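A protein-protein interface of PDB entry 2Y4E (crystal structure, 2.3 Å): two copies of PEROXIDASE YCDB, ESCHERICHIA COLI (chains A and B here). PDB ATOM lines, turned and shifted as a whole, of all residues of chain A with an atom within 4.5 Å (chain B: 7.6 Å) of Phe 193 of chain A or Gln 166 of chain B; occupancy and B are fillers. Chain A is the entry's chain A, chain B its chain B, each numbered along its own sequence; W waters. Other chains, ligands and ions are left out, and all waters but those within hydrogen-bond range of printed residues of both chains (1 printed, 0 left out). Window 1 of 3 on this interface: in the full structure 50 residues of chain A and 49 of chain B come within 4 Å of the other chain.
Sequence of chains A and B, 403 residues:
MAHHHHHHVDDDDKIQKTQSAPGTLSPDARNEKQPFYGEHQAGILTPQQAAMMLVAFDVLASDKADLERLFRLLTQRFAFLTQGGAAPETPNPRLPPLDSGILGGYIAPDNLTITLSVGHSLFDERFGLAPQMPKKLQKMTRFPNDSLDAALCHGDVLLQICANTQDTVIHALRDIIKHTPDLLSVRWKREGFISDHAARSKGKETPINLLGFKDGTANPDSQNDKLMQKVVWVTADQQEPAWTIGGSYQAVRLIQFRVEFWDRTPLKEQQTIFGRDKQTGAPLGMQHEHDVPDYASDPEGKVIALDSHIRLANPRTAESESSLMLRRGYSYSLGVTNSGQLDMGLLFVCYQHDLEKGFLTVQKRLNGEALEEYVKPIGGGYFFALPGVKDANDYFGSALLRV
Printed residues of chain A within 4 Å of Ile 102 of chain B: Leu 210. Of chain A, only Phe 193 comes within 4 Å of Gln 166 of chain B. Printed residues of chain A within 4 Å of Asp 167 of chain B: Ser 195 (3.0 Å). Of the printed residues of chain A, Ile 170 of chain B touches Phe 193 and Ser 333. Printed residues of chain A within 4 Å of Lys 189 of chain B: Ser 333 (3.1 Å). Of the printed residues of chain A, Glu 191 of chain B touches Ser 333 (2.7 Å). The nearest residue of chain A that does not touch Gln 166 of chain B is Ser 333 of chain A (4.3 Å). The nearest printed residue of chain B that does not touch Ser 333 of chain A is Gln 166 of chain B (4.3 Å).
Positions printed for both chains: 50, 192 and 193. Of the 7 pairs that touch across the chains among the printed residues, none has its exchanged pair printed and touching as well.
NZ of Lys 189 of chain B is in salt-bridge range of OE2 of Glu 191 of chain B, 2.7 Å away. The backbone NH (N) of Phe 193 of chain A lies within hydrogen-bond range of the backbone carbonyl oxygen (O) of Ser 331 of chain A (2.8 Å). NE2 of Gln 166 of chain B sits at hydrogen-bond distance from OE1 of Glu 191 of chain B, at 2.7 Å.
The side-chain carboxylate (OE2) of Glu 191 of chain B is in hydrogen-bond range of the side-chain hydroxyl (OG) of Ser 333 of chain A (2.7 Å). OG of Ser 333 of chain A is in hydrogen-bond range of NZ of Lys 189 of chain B, at 3.1 Å.
Water W1 lies within hydrogen-bond range of the side-chain amino group of Lys 189 of chain B and the side-chain hydroxyl of Ser 333 of chain A.
Among the printed residues, merely in contact across the chains: Ser 195 of chain A with Asp 167 of chain B (3.0 Å), Phe 193 of chain A with Gln 166 of chain B (3.4 Å), Leu 210 of chain A with Ile 102 of chain B (3.8 Å), Ser 333 of chain A with Ile 170 of chain B (3.9 Å) and Phe 193 of chain A with Ile 170 of chain B (3.9 Å).
Of the 22 printed residues of chain B, 6 touch a printed residue of chain A. Along chain B the printed residues that touch a printed residue of chain A span positions 102 to 191. Of the 10 printed residues of chain A, 4 touch a printed residue of chain B. Among the printed residues, 7 pairs touch across the chains. Among the printed residues, no Asp or Glu carboxylate lies within 4 Å of a Lys or Arg side-chain nitrogen of the other chain.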
ATOM      1  N   ALA A  50       8.627   3.665  24.028  1.00  0.00           N
ATOM      2  CA  ALA A  50       9.051   4.555  22.966  1.00  0.00           C
ATOM      3  C   ALA A  50      10.326   5.367  23.243  1.00  0.00           C
ATOM      4  O   ALA A  50      10.999   5.770  22.293  1.00  0.00           O
ATOM      5  CB  ALA A  50       7.901   5.463  22.544  1.00  0.00           C
ATOM      6  N   GLY A 192      17.591   7.550  23.268  1.00  0.00           N
ATOM      7  CA  GLY A 192      17.150   6.813  22.090  1.00  0.00           C
ATOM      8  C   GLY A 192      15.644   6.774  21.979  1.00  0.00           C
ATOM      9  O   GLY A 192      14.931   7.271  22.856  1.00  0.00           O
ATOM     10  N   PHE A 193      15.162   6.181  20.893  1.00  0.00           N
ATOM     11  CA  PHE A 193      13.735   6.109  20.620  1.00  0.00           C
ATOM     12  C   PHE A 193      13.479   4.959  19.683  1.00  0.00           C
ATOM     13  O   PHE A 193      14.357   4.594  18.900  1.00  0.00           O
ATOM     14  CB  PHE A 193      13.231   7.417  19.996  1.00  0.00           C
ATOM     15  CG  PHE A 193      13.782   7.690  18.609  1.00  0.00           C
ATOM     16  CD1 PHE A 193      14.971   8.387  18.444  1.00  0.00           C
ATOM     17  CD2 PHE A 193      13.098   7.266  17.473  1.00  0.00           C
ATOM     18  CE1 PHE A 193      15.487   8.654  17.158  1.00  0.00           C
ATOM     19  CE2 PHE A 193      13.599   7.539  16.176  1.00  0.00           C
ATOM     20  CZ  PHE A 193      14.792   8.227  16.021  1.00  0.00           C
ATOM     21  N   ILE A 194      12.289   4.378  19.744  1.00  0.00           N
ATOM     22  CA  ILE A 194      11.916   3.466  18.671  1.00  0.00           C
ATOM     23  C   ILE A 194      10.831   4.058  17.807  1.00  0.00           C
ATOM     24  O   ILE A 194      10.122   4.969  18.234  1.00  0.00           O
ATOM     25  CB  ILE A 194      11.521   2.064  19.116  1.00  0.00           C
ATOM     26  CG1 ILE A 194      10.361   2.129  20.098  1.00  0.00           C
ATOM     27  CG2 ILE A 194      12.723   1.308  19.624  1.00  0.00           C
ATOM     28  CD1 ILE A 194       9.424   1.023  19.889  1.00  0.00           C
ATOM     29  N   SER A 195      10.731   3.510  16.593  1.00  0.00           N
ATOM     30  CA  SER A 195       9.970   4.114  15.505  1.00  0.00           C
ATOM     31  C   SER A 195       8.484   4.236  15.835  1.00  0.00           C
ATOM     32  O   SER A 195       7.857   3.280  16.262  1.00  0.00           O
ATOM     33  CB  SER A 195      10.238   3.410  14.153  1.00  0.00           C
ATOM     34  OG  SER A 195      10.425   1.998  14.281  1.00  0.00           O
ATOM     35  N   LEU A 210      17.221   3.420  11.714  1.00  0.00           N
ATOM     36  CA  LEU A 210      17.475   4.608  10.877  1.00  0.00           C
ATOM     37  C   LEU A 210      18.107   4.295   9.516  1.00  0.00           C
ATOM     38  O   LEU A 210      18.350   5.195   8.694  1.00  0.00           O
ATOM     39  CB  LEU A 210      18.228   5.686  11.659  1.00  0.00           C
ATOM     40  CG  LEU A 210      17.408   6.342  12.791  1.00  0.00           C
ATOM     41  CD1 LEU A 210      18.248   7.198  13.706  1.00  0.00           C
ATOM     42  CD2 LEU A 210      16.187   7.146  12.282  1.00  0.00           C
ATOM     43  N   TYR A 330      17.635   0.682  20.342  1.00  0.00           N
ATOM     44  CA  TYR A 330      16.902   1.931  20.047  1.00  0.00           C
ATOM     45  C   TYR A 330      17.663   2.774  19.031  1.00  0.00           C
ATOM     46  O   TYR A 330      18.882   2.761  19.015  1.00  0.00           O
ATOM     47  CB  TYR A 330      16.732   2.791  21.317  1.00  0.00           C
ATOM     48  CG  TYR A 330      15.647   2.325  22.241  1.00  0.00           C
ATOM     49  CD1 TYR A 330      15.827   1.211  23.037  1.00  0.00           C
ATOM     50  CD2 TYR A 330      14.424   3.014  22.329  1.00  0.00           C
ATOM     51  CE1 TYR A 330      14.819   0.767  23.902  1.00  0.00           C
ATOM     52  CE2 TYR A 330      13.414   2.575  23.171  1.00  0.00           C
ATOM     53  CZ  TYR A 330      13.620   1.442  23.957  1.00  0.00           C
ATOM     54  OH  TYR A 330      12.639   0.976  24.810  1.00  0.00           O
ATOM     55  N   SER A 331      16.940   3.516  18.204  1.00  0.00           N
ATOM     56  CA  SER A 331      17.528   4.528  17.337  1.00  0.00           C
ATOM     57  C   SER A 331      17.933   5.753  18.157  1.00  0.00           C
ATOM     58  O   SER A 331      17.388   5.989  19.259  1.00  0.00           O
ATOM     59  CB  SER A 331      16.520   4.950  16.260  1.00  0.00           C
ATOM     60  OG  SER A 331      16.294   3.883  15.355  1.00  0.00           O
ATOM     61  N   TYR A 332      18.915   6.500  17.643  1.00  0.00           N
ATOM     62  CA  TYR A 332      19.272   7.804  18.217  1.00  0.00           C
ATOM     63  C   TYR A 332      19.582   8.778  17.117  1.00  0.00           C
ATOM     64  O   TYR A 332      19.992   8.388  16.047  1.00  0.00           O
ATOM     65  CB  TYR A 332      20.456   7.694  19.187  1.00  0.00           C
ATOM     66  CG  TYR A 332      21.842   7.695  18.546  1.00  0.00           C
ATOM     67  CD1 TYR A 332      22.489   8.896  18.257  1.00  0.00           C
ATOM     68  CD2 TYR A 332      22.514   6.496  18.265  1.00  0.00           C
ATOM     69  CE1 TYR A 332      23.742   8.908  17.668  1.00  0.00           C
ATOM     70  CE2 TYR A 332      23.778   6.505  17.700  1.00  0.00           C
ATOM     71  CZ  TYR A 332      24.378   7.734  17.390  1.00  0.00           C
ATOM     72  OH  TYR A 332      25.640   7.780  16.830  1.00  0.00           O
ATOM     73  N   SER A 333      19.409  10.051  17.401  1.00  0.00           N
ATOM     74  CA  SER A 333      19.798  11.093  16.487  1.00  0.00           C
ATOM     75  C   SER A 333      20.210  12.281  17.319  1.00  0.00           C
ATOM     76  O   SER A 333      19.408  12.758  18.114  1.00  0.00           O
ATOM     77  CB  SER A 333      18.621  11.461  15.587  1.00  0.00           C
ATOM     78  OG  SER A 333      18.895  12.622  14.838  1.00  0.00           O
ATOM     79  N   ALA B  50       4.815  18.407  19.003  1.00  0.00           N
ATOM     80  CA  ALA B  50       5.605  17.779  20.068  1.00  0.00           C
ATOM     81  C   ALA B  50       7.131  17.751  19.812  1.00  0.00           C
ATOM     82  O   ALA B  50       7.929  17.898  20.752  1.00  0.00           O
ATOM     83  CB  ALA B  50       5.083  16.356  20.369  1.00  0.00           C
ATOM     84  N   ALA B  51       7.518  17.540  18.557  1.00  0.00           N
ATOM     85  CA  ALA B  51       8.921  17.400  18.190  1.00  0.00           C
ATOM     86  C   ALA B  51       9.312  18.488  17.229  1.00  0.00           C
ATOM     87  O   ALA B  51       8.494  18.943  16.434  1.00  0.00           O
ATOM     88  CB  ALA B  51       9.191  16.020  17.566  1.00  0.00           C
ATOM     89  N   MET B  52      10.573  18.898  17.300  1.00  0.00           N
ATOM     90  CA  MET B  52      11.117  19.874  16.395  1.00  0.00           C
ATOM     91  C   MET B  52      12.568  19.510  16.051  1.00  0.00           C
ATOM     92  O   MET B  52      13.247  18.793  16.794  1.00  0.00           O
ATOM     93  CB  MET B  52      11.048  21.270  17.040  1.00  0.00           C
ATOM     94  CG  MET B  52      11.593  22.422  16.163  1.00  0.00           C
ATOM     95  SD  MET B  52      12.549  23.626  17.114  1.00  0.00           S
ATOM     96  CE  MET B  52      13.461  22.429  18.078  1.00  0.00           C
ATOM     97  N   MET B  53      13.012  20.007  14.906  1.00  0.00           N
ATOM     98  CA  MET B  53      14.421  20.038  14.543  1.00  0.00           C
ATOM     99  C   MET B  53      14.734  21.396  13.978  1.00  0.00           C
ATOM    100  O   MET B  53      14.003  21.879  13.138  1.00  0.00           O
ATOM    101  CB  MET B  53      14.741  18.957  13.511  1.00  0.00           C
ATOM    102  CG  MET B  53      16.123  19.074  12.910  1.00  0.00           C
ATOM    103  SD  MET B  53      16.340  17.926  11.562  1.00  0.00           S
ATOM    104  CE  MET B  53      15.953  16.328  12.267  1.00  0.00           C
ATOM    105  N   ILE B 102      12.164   5.012   6.506  1.00  0.00           N
ATOM    106  CA  ILE B 102      12.159   5.005   7.985  1.00  0.00           C
ATOM    107  C   ILE B 102      10.757   5.226   8.564  1.00  0.00           C
ATOM    108  O   ILE B 102      10.545   5.156   9.781  1.00  0.00           O
ATOM    109  CB  ILE B 102      13.176   6.010   8.615  1.00  0.00           C
ATOM    110  CG1 ILE B 102      12.727   7.463   8.426  1.00  0.00           C
ATOM    111  CG2 ILE B 102      14.622   5.752   8.099  1.00  0.00           C
ATOM    112  CD1 ILE B 102      13.451   8.450   9.351  1.00  0.00           C
ATOM    113  N   LEU B 103       9.809   5.455   7.668  1.00  0.00           N
ATOM    114  CA  LEU B 103       8.426   5.679   8.025  1.00  0.00           C
ATOM    115  C   LEU B 103       7.533   4.557   7.535  1.00  0.00           C
ATOM    116  O   LEU B 103       6.339   4.574   7.796  1.00  0.00           O
ATOM    117  CB  LEU B 103       7.952   7.002   7.447  1.00  0.00           C
ATOM    118  CG  LEU B 103       8.449   8.239   8.179  1.00  0.00           C
ATOM    119  CD1 LEU B 103       7.797   9.498   7.618  1.00  0.00           C
ATOM    120  CD2 LEU B 103       8.176   8.070   9.700  1.00  0.00           C
ATOM    121  N   ASP B 110       1.509  13.886   9.659  1.00  0.00           N
ATOM    122  CA  ASP B 110       1.840  13.929  11.091  1.00  0.00           C
ATOM    123  C   ASP B 110       1.994  15.355  11.629  1.00  0.00           C
ATOM    124  O   ASP B 110       2.897  15.628  12.428  1.00  0.00           O
ATOM    125  CB  ASP B 110       3.133  13.134  11.318  1.00  0.00           C
ATOM    126  CG  ASP B 110       3.276  12.602  12.738  1.00  0.00           C
ATOM    127  OD1 ASP B 110       2.247  12.360  13.413  1.00  0.00           O
ATOM    128  OD2 ASP B 110       4.440  12.391  13.168  1.00  0.00           O
ATOM    129  N   ILE B 161      11.751  22.342  11.534  1.00  0.00           N
ATOM    130  CA  ILE B 161      10.956  21.211  11.088  1.00  0.00           C
ATOM    131  C   ILE B 161      10.234  20.688  12.296  1.00  0.00           C
ATOM    132  O   ILE B 161      10.875  20.181  13.231  1.00  0.00           O
ATOM    133  CB  ILE B 161      11.861  20.121  10.453  1.00  0.00           C
ATOM    134  CG1 ILE B 161      12.651  20.701   9.279  1.00  0.00           C
ATOM    135  CG2 ILE B 161      11.072  18.898  10.022  1.00  0.00           C
ATOM    136  CD1 ILE B 161      13.893  19.875   8.876  1.00  0.00           C
ATOM    137  N   ALA B 163       6.883  18.336  13.776  1.00  0.00           N
ATOM    138  CA  ALA B 163       5.829  17.375  13.578  1.00  0.00           C
ATOM    139  C   ALA B 163       5.456  16.800  14.939  1.00  0.00           C
ATOM    140  O   ALA B 163       6.095  17.132  15.963  1.00  0.00           O
ATOM    141  CB  ALA B 163       6.289  16.265  12.622  1.00  0.00           C
ATOM    142  N   ASN B 164       4.428  15.939  14.952  1.00  0.00           N
ATOM    143  CA  ASN B 164       4.032  15.220  16.159  1.00  0.00           C
ATOM    144  C   ASN B 164       5.120  14.300  16.670  1.00  0.00           C
ATOM    145  O   ASN B 164       5.216  14.063  17.874  1.00  0.00           O
ATOM    146  CB  ASN B 164       2.787  14.362  15.924  1.00  0.00           C
ATOM    147  CG  ASN B 164       1.580  15.177  15.516  1.00  0.00           C
ATOM    148  OD1 ASN B 164       1.390  16.318  15.939  1.00  0.00           O
ATOM    149  ND2 ASN B 164       0.756  14.587  14.674  1.00  0.00           N
ATOM    150  N   THR B 165       5.902  13.741  15.748  1.00  0.00           N
ATOM    151  CA  THR B 165       6.910  12.772  16.133  1.00  0.00           C
ATOM    152  C   THR B 165       8.264  13.033  15.471  1.00  0.00           C
ATOM    153  O   THR B 165       8.367  13.576  14.357  1.00  0.00           O
ATOM    154  CB  THR B 165       6.503  11.348  15.810  1.00  0.00           C
ATOM    155  OG1 THR B 165       6.715  11.105  14.418  1.00  0.00           O
ATOM    156  CG2 THR B 165       5.053  11.085  16.177  1.00  0.00           C
ATOM    157  N   GLN B 166       9.293  12.626  16.199  1.00  0.00           N
ATOM    158  CA  GLN B 166      10.673  12.831  15.829  1.00  0.00           C
ATOM    159  C   GLN B 166      10.946  12.051  14.520  1.00  0.00           C
ATOM    160  O   GLN B 166      11.705  12.510  13.665  1.00  0.00           O
ATOM    161  CB  GLN B 166      11.548  12.371  17.017  1.00  0.00           C
ATOM    162  CG  GLN B 166      13.021  12.227  16.753  1.00  0.00           C
ATOM    163  CD  GLN B 166      13.864  11.952  18.019  1.00  0.00           C
ATOM    164  OE1 GLN B 166      13.413  11.323  18.981  1.00  0.00           O
ATOM    165  NE2 GLN B 166      15.103  12.421  17.994  1.00  0.00           N
ATOM    166  N   ASP B 167      10.278  10.906  14.361  1.00  0.00           N
ATOM    167  CA  ASP B 167      10.417  10.050  13.172  1.00  0.00           C
ATOM    168  C   ASP B 167      10.140  10.792  11.886  1.00  0.00           C
ATOM    169  O   ASP B 167      10.865  10.627  10.898  1.00  0.00           O
ATOM    170  CB  ASP B 167       9.434   8.873  13.223  1.00  0.00           C
ATOM    171  CG  ASP B 167       9.485   8.137  14.519  1.00  0.00           C
ATOM    172  OD1 ASP B 167       9.139   8.742  15.565  1.00  0.00           O
ATOM    173  OD2 ASP B 167       9.874   6.946  14.487  1.00  0.00           O
ATOM    174  N   THR B 168       9.070  11.584  11.899  1.00  0.00           N
ATOM    175  CA  THR B 168       8.611  12.325  10.727  1.00  0.00           C
ATOM    176  C   THR B 168       9.577  13.433  10.408  1.00  0.00           C
ATOM    177  O   THR B 168       9.905  13.690   9.260  1.00  0.00           O
ATOM    178  CB  THR B 168       7.185  12.956  10.979  1.00  0.00           C
ATOM    179  OG1 THR B 168       6.236  11.921  11.235  1.00  0.00           O
ATOM    180  CG2 THR B 168       6.711  13.788   9.793  1.00  0.00           C
ATOM    181  N   VAL B 169      10.011  14.112  11.455  1.00  0.00           N
ATOM    182  CA  VAL B 169      10.926  15.246  11.356  1.00  0.00           C
ATOM    183  C   VAL B 169      12.232  14.826  10.672  1.00  0.00           C
ATOM    184  O   VAL B 169      12.697  15.474   9.740  1.00  0.00           O
ATOM    185  CB  VAL B 169      11.172  15.763  12.766  1.00  0.00           C
ATOM    186  CG1 VAL B 169      12.328  16.717  12.831  1.00  0.00           C
ATOM    187  CG2 VAL B 169       9.882  16.414  13.302  1.00  0.00           C
ATOM    188  N   ILE B 170      12.795  13.716  11.139  1.00  0.00           N
ATOM    189  CA  ILE B 170      14.030  13.145  10.600  1.00  0.00           C
ATOM    190  C   ILE B 170      13.845  12.634   9.191  1.00  0.00           C
ATOM    191  O   ILE B 170      14.728  12.823   8.348  1.00  0.00           O
ATOM    192  CB  ILE B 170      14.547  11.984  11.479  1.00  0.00           C
ATOM    193  CG1 ILE B 170      14.975  12.516  12.843  1.00  0.00           C
ATOM    194  CG2 ILE B 170      15.696  11.234  10.779  1.00  0.00           C
ATOM    195  CD1 ILE B 170      15.160  11.449  13.866  1.00  0.00           C
ATOM    196  N   HIS B 171      12.715  11.972   8.933  1.00  0.00           N
ATOM    197  CA  HIS B 171      12.393  11.542   7.562  1.00  0.00           C
ATOM    198  C   HIS B 171      12.416  12.738   6.590  1.00  0.00           C
ATOM    199  O   HIS B 171      13.014  12.661   5.510  1.00  0.00           O
ATOM    200  CB  HIS B 171      11.038  10.834   7.481  1.00  0.00           C
ATOM    201  CG  HIS B 171      10.628  10.527   6.073  1.00  0.00           C
ATOM    202  ND1 HIS B 171       9.841  11.376   5.320  1.00  0.00           N
ATOM    203  CD2 HIS B 171      10.964   9.503   5.257  1.00  0.00           C
ATOM    204  CE1 HIS B 171       9.702  10.876   4.109  1.00  0.00           C
ATOM    205  NE2 HIS B 171      10.377   9.742   4.043  1.00  0.00           N
ATOM    206  N   ALA B 172      11.775  13.836   7.000  1.00  0.00           N
ATOM    207  CA  ALA B 172      11.818  15.101   6.258  1.00  0.00           C
ATOM    208  C   ALA B 172      13.220  15.624   6.001  1.00  0.00           C
ATOM    209  O   ALA B 172      13.545  16.067   4.881  1.00  0.00           O
ATOM    210  CB  ALA B 172      10.984  16.169   6.967  1.00  0.00           C
ATOM    211  N   LYS B 189      22.659  21.381  13.679  1.00  0.00           N
ATOM    212  CA  LYS B 189      21.343  20.792  13.811  1.00  0.00           C
ATOM    213  C   LYS B 189      21.136  20.436  15.255  1.00  0.00           C
ATOM    214  O   LYS B 189      22.058  19.924  15.888  1.00  0.00           O
ATOM    215  CB  LYS B 189      21.219  19.539  12.927  1.00  0.00           C
ATOM    216  CG  LYS B 189      20.065  18.563  13.280  1.00  0.00           C
ATOM    217  CD  LYS B 189      20.420  17.184  12.736  1.00  0.00           C
ATOM    218  CE  LYS B 189      19.453  16.130  13.133  1.00  0.00           C
ATOM    219  NZ  LYS B 189      19.703  15.573  14.488  1.00  0.00           N
ATOM    220  N   GLU B 191      17.733  18.861  17.804  1.00  0.00           N
ATOM    221  CA  GLU B 191      16.384  18.367  17.956  1.00  0.00           C
ATOM    222  C   GLU B 191      15.847  18.641  19.355  1.00  0.00           C
ATOM    223  O   GLU B 191      16.568  18.530  20.360  1.00  0.00           O
ATOM    224  CB  GLU B 191      16.300  16.890  17.622  1.00  0.00           C
ATOM    225  CG  GLU B 191      16.459  16.634  16.129  1.00  0.00           C
ATOM    226  CD  GLU B 191      16.375  15.169  15.777  1.00  0.00           C
ATOM    227  OE1 GLU B 191      15.464  14.498  16.298  1.00  0.00           O
ATOM    228  OE2 GLU B 191      17.217  14.682  14.993  1.00  0.00           O
ATOM    229  N   GLY B 192      14.575  19.028  19.402  1.00  0.00           N
ATOM    230  CA  GLY B 192      13.934  19.436  20.632  1.00  0.00           C
ATOM    231  C   GLY B 192      12.566  18.819  20.772  1.00  0.00           C
ATOM    232  O   GLY B 192      12.093  18.103  19.875  1.00  0.00           O
ATOM    233  N   PHE B 193      11.948  19.080  21.918  1.00  0.00           N
ATOM    234  CA  PHE B 193      10.617  18.557  22.243  1.00  0.00           C
ATOM    235  C   PHE B 193       9.874  19.516  23.182  1.00  0.00           C
ATOM    236  O   PHE B 193      10.495  20.348  23.847  1.00  0.00           O
ATOM    237  CB  PHE B 193      10.718  17.158  22.873  1.00  0.00           C
ATOM    238  CG  PHE B 193      11.382  17.146  24.227  1.00  0.00           C
ATOM    239  CD1 PHE B 193      12.773  17.107  24.345  1.00  0.00           C
ATOM    240  CD2 PHE B 193      10.623  17.164  25.389  1.00  0.00           C
ATOM    241  CE1 PHE B 193      13.381  17.081  25.588  1.00  0.00           C
ATOM    242  CE2 PHE B 193      11.243  17.141  26.647  1.00  0.00           C
ATOM    243  CZ  PHE B 193      12.604  17.105  26.744  1.00  0.00           C
HETATM  244  O   HOH W   1      21.710  13.701  13.730  1.00  0.00           O
